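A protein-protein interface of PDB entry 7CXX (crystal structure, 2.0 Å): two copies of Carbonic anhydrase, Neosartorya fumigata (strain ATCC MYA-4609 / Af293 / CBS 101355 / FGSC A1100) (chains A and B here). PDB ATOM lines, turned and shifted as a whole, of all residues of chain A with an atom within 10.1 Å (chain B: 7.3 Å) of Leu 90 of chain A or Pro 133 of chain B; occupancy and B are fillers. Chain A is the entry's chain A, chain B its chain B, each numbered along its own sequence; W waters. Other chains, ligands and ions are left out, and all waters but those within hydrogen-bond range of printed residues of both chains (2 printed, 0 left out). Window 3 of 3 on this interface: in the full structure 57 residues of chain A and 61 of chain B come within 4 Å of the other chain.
The side-chain amide nitrogen of Asn 91 of chain B lies within hydrogen-bond range of a ring nitrogen (NE2) of His 78 of chain A, 3.1 Å away. OD2 of Asp 89 of chain A is in hydrogen-bond range of ND2 of Asn 91 of chain B. ND2 of Asn 91 of chain A lies within hydrogen-bond range of OD2 of Asp 89 of chain B (2.8 Å). The side-chain carboxylate (OD1) of Asp 89 of chain A lies close to the side-chain carboxylate (OD1) of Asp 89 of chain B (3.4 Å).
ND2 of Asn 80 of chain A is in hydrogen-bond range of NE2 of His 78 of chain A, 3.0 Å away. The side-chain carboxylate (OD1) of Asp 89 of chain A lies within hydrogen-bond range of the backbone NH (N) of Asn 91 of chain A (3.2 Å). The side-chain carboxylate of Asp 89 of chain A lies within hydrogen-bond range of the backbone NH of Val 92 of chain A, at 3.0 Å. The side-chain hydroxyl (OG) of Ser 94 of chain A lies within hydrogen-bond range of the backbone carbonyl oxygen (O) of Leu 90 of chain A (2.7 Å). OD1 of Asp 89 of chain B sits close to N of Asn 91 of chain B (3.2 Å). O of Trp 134 of chain B lies close to OD1 of Asn 137 of chain B.
Asn 80 of chain A touches Asn 91 of chain B. CD2 of Leu 90 of chain A touches CD1 of Leu 130 of chain B, 3.3 Å away. CD1 of Leu 90 of chain A touches CB of Pro 133 of chain B, at 3.9 Å. Asn 91 of chain B touches Asn 91 of chain A (CG to ND2, 3.6 Å). Asn 91 of chain A touches Trp 134 of chain B. Ser 94 of chain A touches Ile 81 of chain B (O to CD1, 2.9 Å). Leu 131 of chain B touches Ser 94 of chain A. Trp 134 of chain B touches Ser 94 of chain A (CB to OG, 3.4 Å). Asn 97 of chain A touches Leu 130 of chain B. Asn 91 of chain B touches Trp 134 of chain A (CB to CH2, 3.6 Å).
Of chain A, only Leu 90 comes within 4 Å of Pro 133 of chain B. No residue of chain A comes within 4 Å of Asn 132 of chain B. Of the printed residues of chain A, Leu 131 of chain B touches Ser 94. Printed residues of chain A within 4 Å of Asp 89 of chain B: Asp 89 (3.4 Å) and Asn 91 (2.8 Å). Of the printed residues of chain A, Ile 81 of chain B touches Ser 94 (2.9 Å), Val 95 (3.5 Å) and Tyr 98 (3.5 Å). Printed residues of chain B within 4 Å of Asn 91 of chain A: Asp 89 (2.8 Å), Asn 91 (3.6 Å) and Trp 134 (3.5 Å). Of the printed residues of chain B, Asn 80 of chain A touches Asn 91. Gly 129 of chain B touches none of the printed residues of chain A. The nearest residue of chain B that does not touch Leu 90 of chain A is Trp 134 of chain B (4.1 Å). The nearest residue of chain A that does not touch Pro 133 of chain B is Ser 94 of chain A (6.3 Å).
Printed residues of chain B that touch a printed residue of chain A: Ile 81, Asp 89, Asn 91, Leu 130, Leu 131, Pro 133 and Trp 134. Printed residues of chain A that touch a printed residue of chain B: His 78, Asn 80, Asp 89, Leu 90, Asn 91, Ser 94, Val 95, Asn 97, Tyr 98 and Trp 134. Hydrophobic or aromatic side chains of chain A that line the printed part of chain B: His 78, Leu 90, Tyr 98 and Trp 134. Among the printed residues, 16 pairs touch across the chains. Among the printed residues, no Asp or Glu carboxylate lies within 4 Å of a Lys or Arg side-chain nitrogen of the other chain.
Asp 89 of chain B touches its own counterpart, Asp 89 of chain A. Asp 89 of chain A touches Asn 91 of chain B, and with the chains exchanged Asn 91 of chain A touches Asp 89 of chain B. Asn 91 of chain A touches its own counterpart, Asn 91 of chain B. Asn 91 of chain A touches Trp 134 of chain B, and with the chains exchanged Trp 134 of chain A touches Asn 91 of chain B. Positions printed for both chains: 84, 86, 89, 91 and 134. Of the 16 pairs that touch across the chains among the printed residues, 6 have their exchanged pair printed and touching as well.
Water W1 lies within hydrogen-bond range of O of Asn 91 of chain B (3.0 Å) and NE1 of Trp 134 of chain A (3.3 Å). Water W2 lies within hydrogen-bond range of the backbone carbonyl oxygen of Asn 91 of chain A (3.0 Å), the backbone NH of Ile 81 of chain B (3.0 Å) and the indole nitrogen of Trp 134 of chain B (3.2 Å).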
ATOM      1  N   HIS A  78      -7.861  13.414   9.359  1.00  0.00           N
ATOM      2  CA  HIS A  78      -6.560  13.725   8.718  1.00  0.00           C
ATOM      3  C   HIS A  78      -6.179  15.150   9.072  1.00  0.00           C
ATOM      4  O   HIS A  78      -6.982  16.049   8.882  1.00  0.00           O
ATOM      5  CB  HIS A  78      -6.641  13.498   7.220  1.00  0.00           C
ATOM      6  CG  HIS A  78      -5.354  13.750   6.529  1.00  0.00           C
ATOM      7  ND1 HIS A  78      -4.267  12.923   6.687  1.00  0.00           N
ATOM      8  CD2 HIS A  78      -4.966  14.732   5.670  1.00  0.00           C
ATOM      9  CE1 HIS A  78      -3.255  13.379   5.933  1.00  0.00           C
ATOM     10  NE2 HIS A  78      -3.661  14.487   5.302  1.00  0.00           N
ATOM     11  N   ASN A  80      -2.886  17.908   8.219  1.00  0.00           N
ATOM     12  CA  ASN A  80      -1.613  18.133   7.490  1.00  0.00           C
ATOM     13  C   ASN A  80      -1.343  19.634   7.490  1.00  0.00           C
ATOM     14  O   ASN A  80      -2.221  20.374   7.964  1.00  0.00           O
ATOM     15  CB  ASN A  80      -1.674  17.446   6.123  1.00  0.00           C
ATOM     16  CG  ASN A  80      -2.604  18.128   5.135  1.00  0.00           C
ATOM     17  OD1 ASN A  80      -2.671  19.338   5.113  1.00  0.00           O
ATOM     18  ND2 ASN A  80      -3.362  17.358   4.381  1.00  0.00           N
ATOM     19  N   LEU A  84      -4.347  20.933   3.280  1.00  0.00           N
ATOM     20  CA  LEU A  84      -4.277  20.761   1.795  1.00  0.00           C
ATOM     21  C   LEU A  84      -4.797  19.404   1.375  1.00  0.00           C
ATOM     22  O   LEU A  84      -4.699  18.443   2.158  1.00  0.00           O
ATOM     23  CB  LEU A  84      -2.818  20.912   1.357  1.00  0.00           C
ATOM     24  CG  LEU A  84      -2.210  22.262   1.681  1.00  0.00           C
ATOM     25  CD1 LEU A  84      -0.792  22.362   1.152  1.00  0.00           C
ATOM     26  CD2 LEU A  84      -3.116  23.372   1.142  1.00  0.00           C
ATOM     27  N   VAL A  85      -5.268  19.348   0.129  1.00  0.00           N
ATOM     28  CA  VAL A  85      -5.592  18.099  -0.579  1.00  0.00           C
ATOM     29  C   VAL A  85      -4.891  18.175  -1.936  1.00  0.00           C
ATOM     30  O   VAL A  85      -5.557  18.348  -2.945  1.00  0.00           O
ATOM     31  CB  VAL A  85      -7.119  17.912  -0.692  1.00  0.00           C
ATOM     32  CG1 VAL A  85      -7.443  16.605  -1.366  1.00  0.00           C
ATOM     33  CG2 VAL A  85      -7.800  17.975   0.686  1.00  0.00           C
ATOM     34  N   PRO A  86      -3.553  18.046  -2.018  1.00  0.00           N
ATOM     35  CA  PRO A  86      -2.869  18.130  -3.312  1.00  0.00           C
ATOM     36  C   PRO A  86      -3.190  16.933  -4.215  1.00  0.00           C
ATOM     37  O   PRO A  86      -3.315  15.839  -3.739  1.00  0.00           O
ATOM     38  CB  PRO A  86      -1.387  18.187  -2.941  1.00  0.00           C
ATOM     39  CG  PRO A  86      -1.411  18.590  -1.464  1.00  0.00           C
ATOM     40  CD  PRO A  86      -2.623  17.876  -0.901  1.00  0.00           C
ATOM     41  N   ASN A  87      -3.168  17.154  -5.538  1.00  0.00           N
ATOM     42  CA  ASN A  87      -3.535  16.147  -6.558  1.00  0.00           C
ATOM     43  C   ASN A  87      -2.764  14.850  -6.364  1.00  0.00           C
ATOM     44  O   ASN A  87      -3.386  13.784  -6.387  1.00  0.00           O
ATOM     45  CB  ASN A  87      -3.251  16.643  -7.982  1.00  0.00           C
ATOM     46  CG  ASN A  87      -4.227  17.704  -8.418  1.00  0.00           C
ATOM     47  OD1 ASN A  87      -5.336  17.784  -7.881  1.00  0.00           O
ATOM     48  ND2 ASN A  87      -3.821  18.505  -9.395  1.00  0.00           N
ATOM     49  N   THR A  88      -1.457  14.932  -6.197  1.00  0.00           N
ATOM     50  CA  THR A  88      -0.561  13.745  -6.286  1.00  0.00           C
ATOM     51  C   THR A  88      -0.091  13.311  -4.901  1.00  0.00           C
ATOM     52  O   THR A  88       0.816  12.478  -4.855  1.00  0.00           O
ATOM     53  CB  THR A  88       0.645  13.971  -7.208  1.00  0.00           C
ATOM     54  OG1 THR A  88       1.488  14.977  -6.639  1.00  0.00           O
ATOM     55  CG2 THR A  88       0.207  14.339  -8.605  1.00  0.00           C
ATOM     56  N   ASP A  89      -0.764  13.755  -3.839  1.00  0.00           N
ATOM     57  CA  ASP A  89      -0.426  13.296  -2.469  1.00  0.00           C
ATOM     58  C   ASP A  89      -1.137  11.967  -2.191  1.00  0.00           C
ATOM     59  O   ASP A  89      -2.306  12.013  -1.851  1.00  0.00           O
ATOM     60  CB  ASP A  89      -0.745  14.374  -1.447  1.00  0.00           C
ATOM     61  CG  ASP A  89      -0.574  13.866  -0.031  1.00  0.00           C
ATOM     62  OD1 ASP A  89       0.392  13.149   0.203  1.00  0.00           O
ATOM     63  OD2 ASP A  89      -1.369  14.237   0.811  1.00  0.00           O
ATOM     64  N   LEU A  90      -0.417  10.861  -2.223  1.00  0.00           N
ATOM     65  CA  LEU A  90      -1.013   9.539  -1.902  1.00  0.00           C
ATOM     66  C   LEU A  90      -1.406   9.443  -0.427  1.00  0.00           C
ATOM     67  O   LEU A  90      -2.252   8.632  -0.150  1.00  0.00           O
ATOM     68  CB  LEU A  90      -0.093   8.377  -2.253  1.00  0.00           C
ATOM     69  CG  LEU A  90      -0.264   7.821  -3.658  1.00  0.00           C
ATOM     70  CD1 LEU A  90       0.689   6.661  -3.907  1.00  0.00           C
ATOM     71  CD2 LEU A  90      -1.690   7.405  -3.930  1.00  0.00           C
ATOM     72  N   ASN A  91      -0.794  10.208   0.460  1.00  0.00           N
ATOM     73  CA  ASN A  91      -1.188  10.263   1.889  1.00  0.00           C
ATOM     74  C   ASN A  91      -2.666  10.689   2.009  1.00  0.00           C
ATOM     75  O   ASN A  91      -3.545   9.838   2.415  1.00  0.00           O
ATOM     76  CB  ASN A  91      -0.172  11.058   2.702  1.00  0.00           C
ATOM     77  CG  ASN A  91      -0.458  11.030   4.206  1.00  0.00           C
ATOM     78  OD1 ASN A  91      -1.614  10.944   4.617  1.00  0.00           O
ATOM     79  ND2 ASN A  91       0.570  11.275   5.003  1.00  0.00           N
ATOM     80  N   VAL A  92      -3.020  11.890   1.590  1.00  0.00           N
ATOM     81  CA  VAL A  92      -4.411  12.390   1.737  1.00  0.00           C
ATOM     82  C   VAL A  92      -5.334  11.627   0.776  1.00  0.00           C
ATOM     83  O   VAL A  92      -6.513  11.436   1.135  1.00  0.00           O
ATOM     84  CB  VAL A  92      -4.512  13.907   1.547  1.00  0.00           C
ATOM     85  CG1 VAL A  92      -4.314  14.324   0.105  1.00  0.00           C
ATOM     86  CG2 VAL A  92      -5.822  14.445   2.065  1.00  0.00           C
ATOM     87  N   MET A  93      -4.857  11.222  -0.409  1.00  0.00           N
ATOM     88  CA  MET A  93      -5.716  10.506  -1.396  1.00  0.00           C
ATOM     89  C   MET A  93      -6.048   9.104  -0.861  1.00  0.00           C
ATOM     90  O   MET A  93      -7.191   8.662  -1.068  1.00  0.00           O
ATOM     91  CB  MET A  93      -5.058  10.459  -2.770  1.00  0.00           C
ATOM     92  CG  MET A  93      -5.064  11.816  -3.485  1.00  0.00           C
ATOM     93  SD  MET A  93      -6.740  12.532  -3.733  1.00  0.00           S
ATOM     94  CE  MET A  93      -6.349  14.274  -3.697  1.00  0.00           C
ATOM     95  N   SER A  94      -5.150   8.485  -0.080  1.00  0.00           N
ATOM     96  CA  SER A  94      -5.420   7.194   0.597  1.00  0.00           C
ATOM     97  C   SER A  94      -6.448   7.411   1.732  1.00  0.00           C
ATOM     98  O   SER A  94      -7.311   6.527   1.914  1.00  0.00           O
ATOM     99  CB  SER A  94      -4.140   6.546   1.126  1.00  0.00           C
ATOM    100  OG  SER A  94      -3.306   6.185   0.025  1.00  0.00           O
ATOM    101  N   VAL A  95      -6.375   8.489   2.507  1.00  0.00           N
ATOM    102  CA  VAL A  95      -7.399   8.687   3.575  1.00  0.00           C
ATOM    103  C   VAL A  95      -8.761   8.915   2.912  1.00  0.00           C
ATOM    104  O   VAL A  95      -9.725   8.284   3.390  1.00  0.00           O
ATOM    105  CB  VAL A  95      -7.103   9.691   4.702  1.00  0.00           C
ATOM    106  CG1 VAL A  95      -5.641   9.879   4.978  1.00  0.00           C
ATOM    107  CG2 VAL A  95      -7.895  10.977   4.645  1.00  0.00           C
ATOM    108  N   ILE A  96      -8.826   9.658   1.801  1.00  0.00           N
ATOM    109  CA  ILE A  96     -10.121   9.943   1.138  1.00  0.00           C
ATOM    110  C   ILE A  96     -10.670   8.637   0.559  1.00  0.00           C
ATOM    111  O   ILE A  96     -11.866   8.343   0.774  1.00  0.00           O
ATOM    112  CB  ILE A  96     -10.012  11.054   0.094  1.00  0.00           C
ATOM    113  CG1 ILE A  96      -9.713  12.376   0.787  1.00  0.00           C
ATOM    114  CG2 ILE A  96     -11.289  11.111  -0.708  1.00  0.00           C
ATOM    115  CD1 ILE A  96      -9.277  13.472  -0.139  1.00  0.00           C
ATOM    116  N   ASN A  97      -9.828   7.874  -0.125  1.00  0.00           N
ATOM    117  CA  ASN A  97     -10.231   6.590  -0.733  1.00  0.00           C
ATOM    118  C   ASN A  97     -10.740   5.631   0.350  1.00  0.00           C
ATOM    119  O   ASN A  97     -11.750   4.960   0.114  1.00  0.00           O
ATOM    120  CB  ASN A  97      -9.086   5.940  -1.497  1.00  0.00           C
ATOM    121  CG  ASN A  97      -9.491   5.587  -2.905  1.00  0.00           C
ATOM    122  OD1 ASN A  97      -9.657   4.408  -3.215  1.00  0.00           O
ATOM    123  ND2 ASN A  97      -9.671   6.607  -3.735  1.00  0.00           N
ATOM    124  N   TYR A  98     -10.033   5.517   1.476  1.00  0.00           N
ATOM    125  CA  TYR A  98     -10.406   4.568   2.548  1.00  0.00           C
ATOM    126  C   TYR A  98     -11.727   5.005   3.213  1.00  0.00           C
ATOM    127  O   TYR A  98     -12.614   4.155   3.466  1.00  0.00           O
ATOM    128  CB  TYR A  98      -9.290   4.492   3.577  1.00  0.00           C
ATOM    129  CG  TYR A  98      -9.503   3.469   4.658  1.00  0.00           C
ATOM    130  CD1 TYR A  98      -9.219   2.130   4.437  1.00  0.00           C
ATOM    131  CD2 TYR A  98      -9.963   3.842   5.907  1.00  0.00           C
ATOM    132  CE1 TYR A  98      -9.376   1.183   5.439  1.00  0.00           C
ATOM    133  CE2 TYR A  98     -10.135   2.914   6.922  1.00  0.00           C
ATOM    134  CZ  TYR A  98      -9.826   1.581   6.686  1.00  0.00           C
ATOM    135  OH  TYR A  98      -9.954   0.637   7.658  1.00  0.00           O
ATOM    136  N   TRP A 134       5.223  21.641  -0.717  1.00  0.00           N
ATOM    137  CA  TRP A 134       3.936  21.483  -0.026  1.00  0.00           C
ATOM    138  C   TRP A 134       3.201  22.834  -0.023  1.00  0.00           C
ATOM    139  O   TRP A 134       2.032  22.913  -0.456  1.00  0.00           O
ATOM    140  CB  TRP A 134       4.177  20.911   1.405  1.00  0.00           C
ATOM    141  CG  TRP A 134       2.892  20.498   2.059  1.00  0.00           C
ATOM    142  CD1 TRP A 134       2.175  21.168   2.989  1.00  0.00           C
ATOM    143  CD2 TRP A 134       2.112  19.353   1.702  1.00  0.00           C
ATOM    144  NE1 TRP A 134       1.010  20.504   3.255  1.00  0.00           N
ATOM    145  CE2 TRP A 134       0.935  19.392   2.484  1.00  0.00           C
ATOM    146  CE3 TRP A 134       2.317  18.273   0.847  1.00  0.00           C
ATOM    147  CZ2 TRP A 134      -0.002  18.362   2.471  1.00  0.00           C
ATOM    148  CZ3 TRP A 134       1.329  17.311   0.755  1.00  0.00           C
ATOM    149  CH2 TRP A 134       0.177  17.372   1.555  1.00  0.00           C
ATOM    150  N   ILE B  81      -3.454   6.767   7.281  1.00  0.00           N
ATOM    151  CA  ILE B  81      -3.806   5.320   7.307  1.00  0.00           C
ATOM    152  C   ILE B  81      -2.608   4.506   7.766  1.00  0.00           C
ATOM    153  O   ILE B  81      -1.515   4.602   7.138  1.00  0.00           O
ATOM    154  CB  ILE B  81      -4.362   4.849   5.959  1.00  0.00           C
ATOM    155  CG1 ILE B  81      -5.678   5.571   5.689  1.00  0.00           C
ATOM    156  CG2 ILE B  81      -4.563   3.347   5.932  1.00  0.00           C
ATOM    157  CD1 ILE B  81      -6.049   5.513   4.263  1.00  0.00           C
ATOM    158  N   LEU B  84       1.854   5.599   9.087  1.00  0.00           N
ATOM    159  CA  LEU B  84       3.065   5.402   8.252  1.00  0.00           C
ATOM    160  C   LEU B  84       3.858   6.703   8.153  1.00  0.00           C
ATOM    161  O   LEU B  84       3.278   7.787   8.255  1.00  0.00           O
ATOM    162  CB  LEU B  84       2.625   4.965   6.856  1.00  0.00           C
ATOM    163  CG  LEU B  84       1.845   3.656   6.812  1.00  0.00           C
ATOM    164  CD1 LEU B  84       1.580   3.252   5.375  1.00  0.00           C
ATOM    165  CD2 LEU B  84       2.572   2.520   7.548  1.00  0.00           C
ATOM    166  N   PRO B  86       6.280   7.050   5.195  1.00  0.00           N
ATOM    167  CA  PRO B  86       7.024   6.551   4.037  1.00  0.00           C
ATOM    168  C   PRO B  86       8.077   7.570   3.562  1.00  0.00           C
ATOM    169  O   PRO B  86       7.877   8.792   3.694  1.00  0.00           O
ATOM    170  CB  PRO B  86       5.908   6.345   3.019  1.00  0.00           C
ATOM    171  CG  PRO B  86       4.610   6.431   3.770  1.00  0.00           C
ATOM    172  CD  PRO B  86       4.878   7.340   4.924  1.00  0.00           C
ATOM    173  N   ASP B  89       6.900  10.425   1.001  1.00  0.00           N
ATOM    174  CA  ASP B  89       5.615  11.075   1.302  1.00  0.00           C
ATOM    175  C   ASP B  89       5.914  12.499   1.764  1.00  0.00           C
ATOM    176  O   ASP B  89       6.241  12.667   2.944  1.00  0.00           O
ATOM    177  CB  ASP B  89       4.781  10.305   2.321  1.00  0.00           C
ATOM    178  CG  ASP B  89       3.544  11.097   2.732  1.00  0.00           C
ATOM    179  OD1 ASP B  89       2.947  11.685   1.862  1.00  0.00           O
ATOM    180  OD2 ASP B  89       3.166  11.076   3.904  1.00  0.00           O
ATOM    181  N   ASN B  91       3.743  14.794   2.366  1.00  0.00           N
ATOM    182  CA  ASN B  91       2.721  15.134   3.387  1.00  0.00           C
ATOM    183  C   ASN B  91       3.353  14.937   4.788  1.00  0.00           C
ATOM    184  O   ASN B  91       3.566  15.952   5.522  1.00  0.00           O
ATOM    185  CB  ASN B  91       1.403  14.418   3.119  1.00  0.00           C
ATOM    186  CG  ASN B  91       0.299  14.798   4.091  1.00  0.00           C
ATOM    187  OD1 ASN B  91       0.565  15.165   5.235  1.00  0.00           O
ATOM    188  ND2 ASN B  91      -0.945  14.652   3.715  1.00  0.00           N
ATOM    189  N   LEU B 128      -6.845  -3.086  -3.481  1.00  0.00           N
ATOM    190  CA  LEU B 128      -7.498  -1.882  -2.891  1.00  0.00           C
ATOM    191  C   LEU B 128      -7.213  -0.653  -3.766  1.00  0.00           C
ATOM    192  O   LEU B 128      -7.298   0.471  -3.253  1.00  0.00           O
ATOM    193  CB  LEU B 128      -7.009  -1.719  -1.448  1.00  0.00           C
ATOM    194  CG  LEU B 128      -7.242  -2.924  -0.533  1.00  0.00           C
ATOM    195  CD1 LEU B 128      -6.859  -2.616   0.899  1.00  0.00           C
ATOM    196  CD2 LEU B 128      -8.687  -3.421  -0.581  1.00  0.00           C
ATOM    197  N   GLY B 129      -6.906  -0.872  -5.053  1.00  0.00           N
ATOM    198  CA  GLY B 129      -6.565   0.173  -6.039  1.00  0.00           C
ATOM    199  C   GLY B 129      -5.488   1.149  -5.572  1.00  0.00           C
ATOM    200  O   GLY B 129      -4.345   0.733  -5.355  1.00  0.00           O
ATOM    201  N   LEU B 130      -5.861   2.420  -5.429  1.00  0.00           N
ATOM    202  CA  LEU B 130      -4.985   3.562  -5.055  1.00  0.00           C
ATOM    203  C   LEU B 130      -4.347   3.285  -3.693  1.00  0.00           C
ATOM    204  O   LEU B 130      -3.247   3.792  -3.446  1.00  0.00           O
ATOM    205  CB  LEU B 130      -5.864   4.818  -5.054  1.00  0.00           C
ATOM    206  CG  LEU B 130      -5.165   6.166  -4.917  1.00  0.00           C
ATOM    207  CD1 LEU B 130      -4.062   6.295  -5.939  1.00  0.00           C
ATOM    208  CD2 LEU B 130      -6.162   7.303  -5.071  1.00  0.00           C
ATOM    209  N   LEU B 131      -4.973   2.448  -2.851  1.00  0.00           N
ATOM    210  CA  LEU B 131      -4.449   2.131  -1.490  1.00  0.00           C
ATOM    211  C   LEU B 131      -3.249   1.182  -1.547  1.00  0.00           C
ATOM    212  O   LEU B 131      -2.512   1.111  -0.526  1.00  0.00           O
ATOM    213  CB  LEU B 131      -5.563   1.514  -0.633  1.00  0.00           C
ATOM    214  CG  LEU B 131      -6.304   2.518   0.245  1.00  0.00           C
ATOM    215  CD1 LEU B 131      -7.612   1.953   0.761  1.00  0.00           C
ATOM    216  CD2 LEU B 131      -5.405   2.930   1.405  1.00  0.00           C
ATOM    217  N   ASN B 132      -3.054   0.440  -2.638  1.00  0.00           N
ATOM    218  CA  ASN B 132      -2.030  -0.642  -2.656  1.00  0.00           C
ATOM    219  C   ASN B 132      -0.672  -0.029  -2.371  1.00  0.00           C
ATOM    220  O   ASN B 132       0.045  -0.544  -1.540  1.00  0.00           O
ATOM    221  CB  ASN B 132      -2.003  -1.453  -3.952  1.00  0.00           C
ATOM    222  CG  ASN B 132      -3.258  -2.272  -4.149  1.00  0.00           C
ATOM    223  OD1 ASN B 132      -3.772  -2.865  -3.197  1.00  0.00           O
ATOM    224  ND2 ASN B 132      -3.768  -2.299  -5.367  1.00  0.00           N
ATOM    225  N   PRO B 133      -0.251   1.044  -3.074  1.00  0.00           N
ATOM    226  CA  PRO B 133       1.072   1.604  -2.835  1.00  0.00           C
ATOM    227  C   PRO B 133       1.254   2.081  -1.386  1.00  0.00           C
ATOM    228  O   PRO B 133       2.355   1.941  -0.899  1.00  0.00           O
ATOM    229  CB  PRO B 133       1.234   2.768  -3.827  1.00  0.00           C
ATOM    230  CG  PRO B 133      -0.051   2.812  -4.641  1.00  0.00           C
ATOM    231  CD  PRO B 133      -0.953   1.683  -4.200  1.00  0.00           C
ATOM    232  N   TRP B 134       0.227   2.701  -0.779  1.00  0.00           N
ATOM    233  CA  TRP B 134       0.274   3.145   0.640  1.00  0.00           C
ATOM    234  C   TRP B 134       0.492   1.927   1.549  1.00  0.00           C
ATOM    235  O   TRP B 134       1.453   1.902   2.344  1.00  0.00           O
ATOM    236  CB  TRP B 134      -0.978   3.942   1.019  1.00  0.00           C
ATOM    237  CG  TRP B 134      -0.811   4.680   2.313  1.00  0.00           C
ATOM    238  CD1 TRP B 134      -1.377   4.389   3.515  1.00  0.00           C
ATOM    239  CD2 TRP B 134       0.016   5.831   2.537  1.00  0.00           C
ATOM    240  NE1 TRP B 134      -0.963   5.271   4.476  1.00  0.00           N
ATOM    241  CE2 TRP B 134      -0.097   6.169   3.903  1.00  0.00           C
ATOM    242  CE3 TRP B 134       0.806   6.632   1.707  1.00  0.00           C
ATOM    243  CZ2 TRP B 134       0.543   7.275   4.453  1.00  0.00           C
ATOM    244  CZ3 TRP B 134       1.458   7.717   2.256  1.00  0.00           C
ATOM    245  CH2 TRP B 134       1.347   8.012   3.610  1.00  0.00           C
ATOM    246  N   LEU B 135      -0.321   0.902   1.396  1.00  0.00           N
ATOM    247  CA  LEU B 135      -0.314  -0.257   2.322  1.00  0.00           C
ATOM    248  C   LEU B 135       0.882  -1.154   2.022  1.00  0.00           C
ATOM    249  O   LEU B 135       1.315  -1.855   2.962  1.00  0.00           O
ATOM    250  CB  LEU B 135      -1.648  -0.998   2.207  1.00  0.00           C
ATOM    251  CG  LEU B 135      -2.867  -0.248   2.732  1.00  0.00           C
ATOM    252  CD1 LEU B 135      -4.085  -1.133   2.583  1.00  0.00           C
ATOM    253  CD2 LEU B 135      -2.688   0.146   4.192  1.00  0.00           C
ATOM    254  N   ARG B 136       1.506  -1.030   0.846  1.00  0.00           N
ATOM    255  CA  ARG B 136       2.774  -1.749   0.515  1.00  0.00           C
ATOM    256  C   ARG B 136       3.794  -1.470   1.609  1.00  0.00           C
ATOM    257  O   ARG B 136       4.615  -2.364   1.908  1.00  0.00           O
ATOM    258  CB  ARG B 136       3.332  -1.357  -0.863  1.00  0.00           C
ATOM    259  CG  ARG B 136       4.285  -2.365  -1.502  1.00  0.00           C
ATOM    260  CD  ARG B 136       4.262  -2.368  -3.038  1.00  0.00           C
ATOM    261  NE  ARG B 136       2.916  -2.492  -3.621  1.00  0.00           N
ATOM    262  CZ  ARG B 136       2.369  -1.705  -4.565  1.00  0.00           C
ATOM    263  NH1 ARG B 136       3.042  -0.705  -5.124  1.00  0.00           N
ATOM    264  NH2 ARG B 136       1.136  -1.955  -4.973  1.00  0.00           N
ATOM    265  N   ASN B 137       3.779  -0.275   2.198  1.00  0.00           N
ATOM    266  CA  ASN B 137       4.704   0.104   3.291  1.00  0.00           C
ATOM    267  C   ASN B 137       4.528  -0.883   4.473  1.00  0.00           C
ATOM    268  O   ASN B 137       5.518  -1.230   5.122  1.00  0.00           O
ATOM    269  CB  ASN B 137       4.498   1.573   3.645  1.00  0.00           C
ATOM    270  CG  ASN B 137       4.886   2.495   2.504  1.00  0.00           C
ATOM    271  OD1 ASN B 137       4.050   3.188   1.917  1.00  0.00           O
ATOM    272  ND2 ASN B 137       6.134   2.417   2.114  1.00  0.00           N
ATOM    273  N   VAL B 138       3.302  -1.282   4.780  1.00  0.00           N
ATOM    274  CA  VAL B 138       3.016  -2.268   5.871  1.00  0.00           C
ATOM    275  C   VAL B 138       3.612  -3.637   5.500  1.00  0.00           C
ATOM    276  O   VAL B 138       4.276  -4.249   6.353  1.00  0.00           O
ATOM    277  CB  VAL B 138       1.504  -2.364   6.169  1.00  0.00           C
ATOM    278  CG1 VAL B 138       1.239  -3.427   7.227  1.00  0.00           C
ATOM    279  CG2 VAL B 138       0.922  -1.018   6.614  1.00  0.00           C
ATOM    280  N   ASP B 140       6.152  -4.261   3.583  1.00  0.00           N
ATOM    281  CA  ASP B 140       7.621  -4.148   3.719  1.00  0.00           C
ATOM    282  C   ASP B 140       8.036  -4.378   5.173  1.00  0.00           C
ATOM    283  O   ASP B 140       9.159  -4.864   5.425  1.00  0.00           O
ATOM    284  CB  ASP B 140       8.157  -2.793   3.234  1.00  0.00           C
ATOM    285  CG  ASP B 140       8.083  -2.613   1.719  1.00  0.00           C
ATOM    286  OD1 ASP B 140       7.765  -3.593   1.028  1.00  0.00           O
ATOM    287  OD2 ASP B 140       8.334  -1.484   1.249  1.00  0.00           O
HETATM  288  O   HOH W   1       1.728  18.279   5.602  1.00  0.00           O
HETATM  289  O   HOH W   2      -2.971   7.821   4.521  1.00  0.00           O
